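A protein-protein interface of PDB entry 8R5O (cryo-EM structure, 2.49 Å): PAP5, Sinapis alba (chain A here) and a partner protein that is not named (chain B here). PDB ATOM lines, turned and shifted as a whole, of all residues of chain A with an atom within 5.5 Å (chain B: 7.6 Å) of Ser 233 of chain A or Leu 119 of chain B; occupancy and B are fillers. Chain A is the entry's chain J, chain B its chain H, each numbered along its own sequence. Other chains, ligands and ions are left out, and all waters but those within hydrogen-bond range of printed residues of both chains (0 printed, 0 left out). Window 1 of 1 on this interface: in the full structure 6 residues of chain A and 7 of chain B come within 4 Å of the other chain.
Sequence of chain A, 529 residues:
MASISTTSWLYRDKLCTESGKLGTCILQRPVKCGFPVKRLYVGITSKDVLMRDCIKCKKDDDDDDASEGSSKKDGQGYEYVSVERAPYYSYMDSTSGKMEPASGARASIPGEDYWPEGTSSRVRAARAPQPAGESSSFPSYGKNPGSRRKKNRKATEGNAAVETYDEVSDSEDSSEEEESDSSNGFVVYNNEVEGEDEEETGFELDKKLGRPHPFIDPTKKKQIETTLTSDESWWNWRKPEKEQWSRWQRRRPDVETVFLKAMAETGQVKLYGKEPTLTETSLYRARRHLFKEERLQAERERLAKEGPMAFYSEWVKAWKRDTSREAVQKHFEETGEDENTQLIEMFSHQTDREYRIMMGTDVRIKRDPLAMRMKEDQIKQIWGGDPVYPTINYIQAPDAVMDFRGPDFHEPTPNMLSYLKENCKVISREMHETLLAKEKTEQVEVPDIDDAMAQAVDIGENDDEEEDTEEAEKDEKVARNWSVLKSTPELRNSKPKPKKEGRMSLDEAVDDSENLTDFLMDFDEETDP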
ATOM      1  N   LEU A 228      22.156  21.481   5.667  1.00  0.00           N
ATOM      2  CA  LEU A 228      20.774  21.330   6.106  1.00  0.00           C
ATOM      3  C   LEU A 228      20.160  22.682   6.444  1.00  0.00           C
ATOM      4  O   LEU A 228      20.779  23.519   7.107  1.00  0.00           O
ATOM      5  CB  LEU A 228      20.708  20.397   7.316  1.00  0.00           C
ATOM      6  CG  LEU A 228      21.338  19.015   7.122  1.00  0.00           C
ATOM      7  CD1 LEU A 228      21.238  18.193   8.394  1.00  0.00           C
ATOM      8  CD2 LEU A 228      20.690  18.285   5.957  1.00  0.00           C
ATOM      9  N   SER A 230      17.321  23.549   8.211  1.00  0.00           N
ATOM     10  CA  SER A 230      16.422  23.619   9.361  1.00  0.00           C
ATOM     11  C   SER A 230      15.116  22.866   9.131  1.00  0.00           C
ATOM     12  O   SER A 230      14.328  22.688  10.065  1.00  0.00           O
ATOM     13  CB  SER A 230      16.132  25.076   9.735  1.00  0.00           C
ATOM     14  OG  SER A 230      15.198  25.154  10.796  1.00  0.00           O
ATOM     15  N   ASP A 231      14.881  22.410   7.902  1.00  0.00           N
ATOM     16  CA  ASP A 231      13.737  21.562   7.600  1.00  0.00           C
ATOM     17  C   ASP A 231      14.132  20.107   7.401  1.00  0.00           C
ATOM     18  O   ASP A 231      13.285  19.222   7.557  1.00  0.00           O
ATOM     19  CB  ASP A 231      13.009  22.078   6.353  1.00  0.00           C
ATOM     20  CG  ASP A 231      11.555  21.655   6.304  1.00  0.00           C
ATOM     21  OD1 ASP A 231      11.283  20.449   6.125  1.00  0.00           O
ATOM     22  OD2 ASP A 231      10.677  22.530   6.456  1.00  0.00           O
ATOM     23  N   GLU A 232      15.393  19.845   7.070  1.00  0.00           N
ATOM     24  CA  GLU A 232      15.939  18.499   7.030  1.00  0.00           C
ATOM     25  C   GLU A 232      16.724  18.165   8.289  1.00  0.00           C
ATOM     26  O   GLU A 232      17.448  17.166   8.312  1.00  0.00           O
ATOM     27  CB  GLU A 232      16.836  18.321   5.802  1.00  0.00           C
ATOM     28  CG  GLU A 232      16.313  18.958   4.525  1.00  0.00           C
ATOM     29  CD  GLU A 232      16.800  20.382   4.343  1.00  0.00           C
ATOM     30  OE1 GLU A 232      16.730  21.165   5.312  1.00  0.00           O
ATOM     31  OE2 GLU A 232      17.264  20.714   3.232  1.00  0.00           O
ATOM     32  N   SER A 233      16.599  18.979   9.332  1.00  0.00           N
ATOM     33  CA  SER A 233      17.400  18.852  10.537  1.00  0.00           C
ATOM     34  C   SER A 233      16.530  18.510  11.739  1.00  0.00           C
ATOM     35  O   SER A 233      15.361  18.898  11.815  1.00  0.00           O
ATOM     36  CB  SER A 233      18.170  20.145  10.819  1.00  0.00           C
ATOM     37  OG  SER A 233      18.863  20.064  12.053  1.00  0.00           O
ATOM     38  N   TRP A 234      17.119  17.774  12.676  1.00  0.00           N
ATOM     39  CA  TRP A 234      16.480  17.528  13.957  1.00  0.00           C
ATOM     40  C   TRP A 234      16.359  18.831  14.743  1.00  0.00           C
ATOM     41  O   TRP A 234      17.008  19.835  14.440  1.00  0.00           O
ATOM     42  CB  TRP A 234      17.274  16.504  14.764  1.00  0.00           C
ATOM     43  CG  TRP A 234      17.438  15.187  14.084  1.00  0.00           C
ATOM     44  CD1 TRP A 234      16.566  14.591  13.223  1.00  0.00           C
ATOM     45  CD2 TRP A 234      18.556  14.301  14.201  1.00  0.00           C
ATOM     46  NE1 TRP A 234      17.068  13.385  12.802  1.00  0.00           N
ATOM     47  CE2 TRP A 234      18.290  13.184  13.387  1.00  0.00           C
ATOM     48  CE3 TRP A 234      19.754  14.344  14.917  1.00  0.00           C
ATOM     49  CZ2 TRP A 234      19.179  12.120  13.270  1.00  0.00           C
ATOM     50  CZ3 TRP A 234      20.634  13.288  14.800  1.00  0.00           C
ATOM     51  CH2 TRP A 234      20.343  12.191  13.984  1.00  0.00           C
ATOM     52  N   TRP A 235      15.515  18.800  15.776  1.00  0.00           N
ATOM     53  CA  TRP A 235      15.234  20.010  16.540  1.00  0.00           C
ATOM     54  C   TRP A 235      16.482  20.540  17.239  1.00  0.00           C
ATOM     55  O   TRP A 235      16.682  21.757  17.324  1.00  0.00           O
ATOM     56  CB  TRP A 235      14.121  19.743  17.554  1.00  0.00           C
ATOM     57  CG  TRP A 235      14.446  18.681  18.562  1.00  0.00           C
ATOM     58  CD1 TRP A 235      14.218  17.345  18.443  1.00  0.00           C
ATOM     59  CD2 TRP A 235      15.051  18.872  19.845  1.00  0.00           C
ATOM     60  NE1 TRP A 235      14.645  16.689  19.571  1.00  0.00           N
ATOM     61  CE2 TRP A 235      15.162  17.606  20.447  1.00  0.00           C
ATOM     62  CE3 TRP A 235      15.514  19.992  20.541  1.00  0.00           C
ATOM     63  CZ2 TRP A 235      15.713  17.428  21.714  1.00  0.00           C
ATOM     64  CZ3 TRP A 235      16.062  19.813  21.796  1.00  0.00           C
ATOM     65  CH2 TRP A 235      16.157  18.542  22.370  1.00  0.00           C
ATOM     66  N   TRP A 237      19.540  20.562  16.333  1.00  0.00           N
ATOM     67  CA  TRP A 237      20.546  21.139  15.447  1.00  0.00           C
ATOM     68  C   TRP A 237      20.017  22.310  14.628  1.00  0.00           C
ATOM     69  O   TRP A 237      20.711  22.775  13.718  1.00  0.00           O
ATOM     70  CB  TRP A 237      21.117  20.070  14.515  1.00  0.00           C
ATOM     71  CG  TRP A 237      21.941  19.028  15.208  1.00  0.00           C
ATOM     72  CD1 TRP A 237      21.729  17.685  15.202  1.00  0.00           C
ATOM     73  CD2 TRP A 237      23.103  19.247  16.017  1.00  0.00           C
ATOM     74  NE1 TRP A 237      22.688  17.049  15.950  1.00  0.00           N
ATOM     75  CE2 TRP A 237      23.543  17.987  16.462  1.00  0.00           C
ATOM     76  CE3 TRP A 237      23.815  20.386  16.406  1.00  0.00           C
ATOM     77  CZ2 TRP A 237      24.663  17.833  17.277  1.00  0.00           C
ATOM     78  CZ3 TRP A 237      24.924  20.231  17.212  1.00  0.00           C
ATOM     79  CH2 TRP A 237      25.338  18.964  17.640  1.00  0.00           C
ATOM     80  N   ARG A 238      18.817  22.796  14.921  1.00  0.00           N
ATOM     81  CA  ARG A 238      18.262  23.926  14.189  1.00  0.00           C
ATOM     82  C   ARG A 238      18.750  25.242  14.779  1.00  0.00           C
ATOM     83  O   ARG A 238      18.908  25.376  15.995  1.00  0.00           O
ATOM     84  CB  ARG A 238      16.737  23.883  14.210  1.00  0.00           C
ATOM     85  CG  ARG A 238      16.144  22.739  13.423  1.00  0.00           C
ATOM     86  CD  ARG A 238      14.669  22.581  13.718  1.00  0.00           C
ATOM     87  NE  ARG A 238      14.147  21.329  13.188  1.00  0.00           N
ATOM     88  CZ  ARG A 238      12.983  20.798  13.534  1.00  0.00           C
ATOM     89  NH1 ARG A 238      12.188  21.387  14.410  1.00  0.00           N
ATOM     90  NH2 ARG A 238      12.612  19.643  12.991  1.00  0.00           N
ATOM     91  N   THR B  89       3.408  17.210  19.141  1.00  0.00           N
ATOM     92  CA  THR B  89       4.384  17.547  18.123  1.00  0.00           C
ATOM     93  C   THR B  89       5.238  16.321  17.808  1.00  0.00           C
ATOM     94  O   THR B  89       5.260  15.359  18.579  1.00  0.00           O
ATOM     95  CB  THR B  89       5.265  18.705  18.593  1.00  0.00           C
ATOM     96  OG1 THR B  89       5.938  18.337  19.804  1.00  0.00           O
ATOM     97  CG2 THR B  89       4.430  19.948  18.838  1.00  0.00           C
ATOM     98  N   PRO B  90       5.936  16.319  16.667  1.00  0.00           N
ATOM     99  CA  PRO B  90       6.824  15.182  16.366  1.00  0.00           C
ATOM    100  C   PRO B  90       7.850  14.904  17.452  1.00  0.00           C
ATOM    101  O   PRO B  90       8.164  13.737  17.715  1.00  0.00           O
ATOM    102  CB  PRO B  90       7.490  15.609  15.052  1.00  0.00           C
ATOM    103  CG  PRO B  90       6.498  16.501  14.410  1.00  0.00           C
ATOM    104  CD  PRO B  90       5.833  17.249  15.529  1.00  0.00           C
ATOM    105  N   GLU B  91       8.387  15.945  18.091  1.00  0.00           N
ATOM    106  CA  GLU B  91       9.336  15.731  19.179  1.00  0.00           C
ATOM    107  C   GLU B  91       8.673  15.044  20.367  1.00  0.00           C
ATOM    108  O   GLU B  91       9.253  14.130  20.962  1.00  0.00           O
ATOM    109  CB  GLU B  91       9.957  17.060  19.608  1.00  0.00           C
ATOM    110  CG  GLU B  91      10.823  17.725  18.551  1.00  0.00           C
ATOM    111  CD  GLU B  91      10.018  18.473  17.506  1.00  0.00           C
ATOM    112  OE1 GLU B  91       8.832  18.766  17.763  1.00  0.00           O
ATOM    113  OE2 GLU B  91      10.571  18.766  16.426  1.00  0.00           O
ATOM    114  N   ALA B  92       7.463  15.474  20.728  1.00  0.00           N
ATOM    115  CA  ALA B  92       6.756  14.841  21.836  1.00  0.00           C
ATOM    116  C   ALA B  92       6.324  13.425  21.480  1.00  0.00           C
ATOM    117  O   ALA B  92       6.363  12.528  22.331  1.00  0.00           O
ATOM    118  CB  ALA B  92       5.550  15.686  22.243  1.00  0.00           C
ATOM    119  N   ASP B  93       5.909  13.205  20.232  1.00  0.00           N
ATOM    120  CA  ASP B  93       5.531  11.863  19.803  1.00  0.00           C
ATOM    121  C   ASP B  93       6.726  10.918  19.824  1.00  0.00           C
ATOM    122  O   ASP B  93       6.594   9.749  20.201  1.00  0.00           O
ATOM    123  CB  ASP B  93       4.910  11.913  18.407  1.00  0.00           C
ATOM    124  CG  ASP B  93       4.391  10.566  17.953  1.00  0.00           C
ATOM    125  OD1 ASP B  93       3.466  10.037  18.601  1.00  0.00           O
ATOM    126  OD2 ASP B  93       4.905  10.038  16.945  1.00  0.00           O
ATOM    127  N   PHE B  94       7.899  11.406  19.418  1.00  0.00           N
ATOM    128  CA  PHE B  94       9.102  10.581  19.455  1.00  0.00           C
ATOM    129  C   PHE B  94       9.516  10.269  20.888  1.00  0.00           C
ATOM    130  O   PHE B  94      10.000   9.168  21.173  1.00  0.00           O
ATOM    131  CB  PHE B  94      10.235  11.279  18.701  1.00  0.00           C
ATOM    132  CG  PHE B  94      11.566  10.598  18.833  1.00  0.00           C
ATOM    133  CD1 PHE B  94      11.781   9.351  18.272  1.00  0.00           C
ATOM    134  CD2 PHE B  94      12.608  11.212  19.505  1.00  0.00           C
ATOM    135  CE1 PHE B  94      13.003   8.727  18.389  1.00  0.00           C
ATOM    136  CE2 PHE B  94      13.837  10.591  19.623  1.00  0.00           C
ATOM    137  CZ  PHE B  94      14.033   9.349  19.066  1.00  0.00           C
ATOM    138  N   ALA B  95       9.332  11.225  21.802  1.00  0.00           N
ATOM    139  CA  ALA B  95       9.757  11.028  23.185  1.00  0.00           C
ATOM    140  C   ALA B  95       9.000   9.885  23.847  1.00  0.00           C
ATOM    141  O   ALA B  95       9.592   9.078  24.571  1.00  0.00           O
ATOM    142  CB  ALA B  95       9.575  12.321  23.979  1.00  0.00           C
ATOM    143  N   LEU B 107      16.678   1.762  18.416  1.00  0.00           N
ATOM    144  CA  LEU B 107      15.226   1.709  18.331  1.00  0.00           C
ATOM    145  C   LEU B 107      14.807   0.570  17.412  1.00  0.00           C
ATOM    146  O   LEU B 107      15.285   0.462  16.280  1.00  0.00           O
ATOM    147  CB  LEU B 107      14.676   3.041  17.827  1.00  0.00           C
ATOM    148  CG  LEU B 107      15.069   4.265  18.657  1.00  0.00           C
ATOM    149  CD1 LEU B 107      14.550   5.538  18.020  1.00  0.00           C
ATOM    150  CD2 LEU B 107      14.568   4.132  20.086  1.00  0.00           C
ATOM    151  N   ALA B 112       8.556   3.665  16.921  1.00  0.00           N
ATOM    152  CA  ALA B 112       9.646   4.561  17.295  1.00  0.00           C
ATOM    153  C   ALA B 112      10.565   4.841  16.113  1.00  0.00           C
ATOM    154  O   ALA B 112      11.096   5.949  15.983  1.00  0.00           O
ATOM    155  CB  ALA B 112      10.436   3.971  18.461  1.00  0.00           C
ATOM    156  N   ILE B 113      10.774   3.847  15.247  1.00  0.00           N
ATOM    157  CA  ILE B 113      11.583   4.063  14.050  1.00  0.00           C
ATOM    158  C   ILE B 113      10.919   5.086  13.140  1.00  0.00           C
ATOM    159  O   ILE B 113      11.577   5.995  12.618  1.00  0.00           O
ATOM    160  CB  ILE B 113      11.833   2.728  13.323  1.00  0.00           C
ATOM    161  CG1 ILE B 113      12.766   1.836  14.144  1.00  0.00           C
ATOM    162  CG2 ILE B 113      12.408   2.971  11.939  1.00  0.00           C
ATOM    163  CD1 ILE B 113      13.006   0.472  13.530  1.00  0.00           C
ATOM    164  N   GLU B 114       9.607   4.958  12.934  1.00  0.00           N
ATOM    165  CA  GLU B 114       8.888   5.943  12.134  1.00  0.00           C
ATOM    166  C   GLU B 114       8.890   7.309  12.808  1.00  0.00           C
ATOM    167  O   GLU B 114       9.043   8.336  12.138  1.00  0.00           O
ATOM    168  CB  GLU B 114       7.459   5.468  11.874  1.00  0.00           C
ATOM    169  CG  GLU B 114       6.585   6.474  11.138  1.00  0.00           C
ATOM    170  CD  GLU B 114       7.051   6.744   9.719  1.00  0.00           C
ATOM    171  OE1 GLU B 114       7.773   5.899   9.150  1.00  0.00           O
ATOM    172  OE2 GLU B 114       6.694   7.808   9.171  1.00  0.00           O
ATOM    173  N   ALA B 115       8.725   7.343  14.134  1.00  0.00           N
ATOM    174  CA  ALA B 115       8.759   8.612  14.851  1.00  0.00           C
ATOM    175  C   ALA B 115      10.122   9.284  14.740  1.00  0.00           C
ATOM    176  O   ALA B 115      10.205  10.516  14.704  1.00  0.00           O
ATOM    177  CB  ALA B 115       8.388   8.401  16.318  1.00  0.00           C
ATOM    178  N   PHE B 116      11.196   8.494  14.691  1.00  0.00           N
ATOM    179  CA  PHE B 116      12.525   9.054  14.462  1.00  0.00           C
ATOM    180  C   PHE B 116      12.609   9.715  13.091  1.00  0.00           C
ATOM    181  O   PHE B 116      13.182  10.801  12.951  1.00  0.00           O
ATOM    182  CB  PHE B 116      13.578   7.955  14.602  1.00  0.00           C
ATOM    183  CG  PHE B 116      14.996   8.455  14.560  1.00  0.00           C
ATOM    184  CD1 PHE B 116      15.655   8.803  15.727  1.00  0.00           C
ATOM    185  CD2 PHE B 116      15.676   8.557  13.357  1.00  0.00           C
ATOM    186  CE1 PHE B 116      16.959   9.253  15.695  1.00  0.00           C
ATOM    187  CE2 PHE B 116      16.980   9.005  13.318  1.00  0.00           C
ATOM    188  CZ  PHE B 116      17.622   9.353  14.489  1.00  0.00           C
ATOM    189  N   LYS B 117      12.039   9.072  12.070  1.00  0.00           N
ATOM    190  CA  LYS B 117      12.035   9.649  10.730  1.00  0.00           C
ATOM    191  C   LYS B 117      11.230  10.940  10.681  1.00  0.00           C
ATOM    192  O   LYS B 117      11.600  11.886   9.978  1.00  0.00           O
ATOM    193  CB  LYS B 117      11.472   8.641   9.729  1.00  0.00           C
ATOM    194  CG  LYS B 117      12.267   7.356   9.604  1.00  0.00           C
ATOM    195  CD  LYS B 117      13.332   7.464   8.530  1.00  0.00           C
ATOM    196  CE  LYS B 117      13.890   6.096   8.185  1.00  0.00           C
ATOM    197  NZ  LYS B 117      12.804   5.145   7.816  1.00  0.00           N
ATOM    198  N   MET B 118      10.121  10.996  11.422  1.00  0.00           N
ATOM    199  CA  MET B 118       9.239  12.155  11.394  1.00  0.00           C
ATOM    200  C   MET B 118       9.822  13.367  12.107  1.00  0.00           C
ATOM    201  O   MET B 118       9.221  14.444  12.047  1.00  0.00           O
ATOM    202  CB  MET B 118       7.885  11.798  12.009  1.00  0.00           C
ATOM    203  CG  MET B 118       7.124  10.724  11.253  1.00  0.00           C
ATOM    204  SD  MET B 118       6.689  11.215   9.576  1.00  0.00           S
ATOM    205  CE  MET B 118       5.580  12.581   9.899  1.00  0.00           C
ATOM    206  N   LEU B 119      10.969  13.224  12.773  1.00  0.00           N
ATOM    207  CA  LEU B 119      11.614  14.361  13.421  1.00  0.00           C
ATOM    208  C   LEU B 119      12.094  15.409  12.427  1.00  0.00           C
ATOM    209  O   LEU B 119      12.418  16.526  12.843  1.00  0.00           O
ATOM    210  CB  LEU B 119      12.789  13.879  14.273  1.00  0.00           C
ATOM    211  CG  LEU B 119      12.427  13.077  15.523  1.00  0.00           C
ATOM    212  CD1 LEU B 119      13.679  12.551  16.203  1.00  0.00           C
ATOM    213  CD2 LEU B 119      11.613  13.931  16.481  1.00  0.00           C
ATOM    214  N   ARG B 120      12.147  15.082  11.138  1.00  0.00           N
ATOM    215  CA  ARG B 120      12.510  16.036  10.103  1.00  0.00           C
ATOM    216  C   ARG B 120      11.276  16.393   9.292  1.00  0.00           C
ATOM    217  O   ARG B 120      10.678  15.501   8.672  1.00  0.00           O
ATOM    218  CB  ARG B 120      13.596  15.459   9.196  1.00  0.00           C
ATOM    219  CG  ARG B 120      14.923  15.238   9.889  1.00  0.00           C
ATOM    220  CD  ARG B 120      15.858  14.414   9.028  1.00  0.00           C
ATOM    221  NE  ARG B 120      17.159  14.239   9.659  1.00  0.00           N
ATOM    222  CZ  ARG B 120      18.069  13.358   9.268  1.00  0.00           C
ATOM    223  NH1 ARG B 120      17.849  12.546   8.248  1.00  0.00           N
ATOM    224  NH2 ARG B 120      19.223  13.286   9.922  1.00  0.00           N
ATOM    225  N   PRO B 121      10.852  17.658   9.272  1.00  0.00           N
ATOM    226  CA  PRO B 121       9.681  18.027   8.459  1.00  0.00           C
ATOM    227  C   PRO B 121       9.860  17.764   6.976  1.00  0.00           C
ATOM    228  O   PRO B 121       8.858  17.616   6.267  1.00  0.00           O
ATOM    229  CB  PRO B 121       9.504  19.525   8.748  1.00  0.00           C
ATOM    230  CG  PRO B 121      10.787  19.970   9.368  1.00  0.00           C
ATOM    231  CD  PRO B 121      11.343  18.785  10.080  1.00  0.00           C
ATOM    232  N   SER B 122      11.098  17.702   6.482  1.00  0.00           N
ATOM    233  CA  SER B 122      11.317  17.349   5.083  1.00  0.00           C
ATOM    234  C   SER B 122      10.851  15.926   4.796  1.00  0.00           C
ATOM    235  O   SER B 122      10.287  15.655   3.732  1.00  0.00           O
ATOM    236  CB  SER B 122      12.792  17.514   4.724  1.00  0.00           C
ATOM    237  OG  SER B 122      13.595  16.602   5.449  1.00  0.00           O
ATOM    238  N   TYR B 123      11.090  15.004   5.730  1.00  0.00           N
ATOM    239  CA  TYR B 123      10.597  13.642   5.566  1.00  0.00           C
ATOM    240  C   TYR B 123       9.074  13.603   5.596  1.00  0.00           C
ATOM    241  O   TYR B 123       8.454  12.817   4.872  1.00  0.00           O
ATOM    242  CB  TYR B 123      11.179  12.739   6.652  1.00  0.00           C
ATOM    243  CG  TYR B 123      10.691  11.310   6.597  1.00  0.00           C
ATOM    244  CD1 TYR B 123      11.334  10.368   5.810  1.00  0.00           C
ATOM    245  CD2 TYR B 123       9.592  10.902   7.340  1.00  0.00           C
ATOM    246  CE1 TYR B 123      10.894   9.060   5.759  1.00  0.00           C
ATOM    247  CE2 TYR B 123       9.144   9.598   7.294  1.00  0.00           C
ATOM    248  CZ  TYR B 123       9.799   8.682   6.504  1.00  0.00           C
ATOM    249  OH  TYR B 123       9.356   7.381   6.457  1.00  0.00           O
ATOM    250  N   ARG B 124       8.459  14.435   6.440  1.00  0.00           N
ATOM    251  CA  ARG B 124       7.003  14.481   6.506  1.00  0.00           C
ATOM    252  C   ARG B 124       6.404  14.947   5.185  1.00  0.00           C
ATOM    253  O   ARG B 124       5.413  14.380   4.712  1.00  0.00           O
ATOM    254  CB  ARG B 124       6.560  15.392   7.651  1.00  0.00           C
ATOM    255  CG  ARG B 124       5.108  15.825   7.562  1.00  0.00           C
ATOM    256  CD  ARG B 124       4.603  16.431   8.860  1.00  0.00           C
ATOM    257  NE  ARG B 124       5.333  17.626   9.265  1.00  0.00           N
ATOM    258  CZ  ARG B 124       6.222  17.663  10.249  1.00  0.00           C
ATOM    259  NH1 ARG B 124       6.528  16.579  10.943  1.00  0.00           N
ATOM    260  NH2 ARG B 124       6.815  18.815  10.544  1.00  0.00           N
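OE2 of Glu 91 of chain B lies within salt-bridge range of NH1 of Arg 238 of chain A (3.7 Å). O of Leu 119 of chain B is in hydrogen-bond range of NH2 of Arg 238 of chain A (3.1 Å). NE of Arg 120 of chain B sits at hydrogen-bond distance from O of Glu 232 of chain A. The backbone NH (N) of Ser 122 of chain B is in hydrogen-bond range of the side-chain carboxylate (OD1) of Asp 231 of chain A (2.8 Å). O of Asp 231 of chain A sits close to N of Pro 121 of chain B (3.4 Å). NE1 of Trp 234 of chain A lies close to NE of Arg 120 of chain B.
The guanidinium group (NE) of Arg 238 of chain A sits at hydrogen-bond distance from the backbone carbonyl oxygen (O) of Ser 230 of chain A, 3.4 Å away. The guanidinium group (NE) of Arg 238 of chain A is in hydrogen-bond range of the backbone carbonyl oxygen (O) of Ser 233 of chain A (3.0 Å). The backbone carbonyl oxygen (O) of Trp 234 of chain A lies close to the guanidinium group (NE) of Arg 238 of chain A (3.5 Å).
Among the printed residues, pairs that only touch across the chains: Arg 238 of chain A with Pro 121 of chain B, Trp 234 of chain A with Phe 116 of chain B, Glu 232 of chain A with Ser 122 of chain B, Trp 235 of chain A with Glu 91 of chain B, Asp 231 of chain A with Arg 120 of chain B, Ser 233 of chain A with Leu 119 of chain B and Trp 234 of chain A with Leu 119 of chain B.
Printed residues of chain B within 4 Å of Ser 233 of chain A: Leu 119. Of the printed residues of chain A, Leu 119 of chain B touches Ser 233, Trp 234 and Arg 238. Of the printed residues of chain A, Ser 122 of chain B touches Asp 231 and Glu 232. Of the printed residues of chain A, Phe 116 of chain B touches Trp 234 (3.4 Å). The nearest residue of chain B that does not touch Ser 233 of chain A is Arg 120 of chain B (4.1 Å). The nearest printed residue of chain A that does not touch Leu 119 of chain B is Trp 235 of chain A (4.7 Å).
Hydrophobic or aromatic side chains of chain B within 4 Å of the printed part of chain A: Phe 116, Leu 119 and Pro 121.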
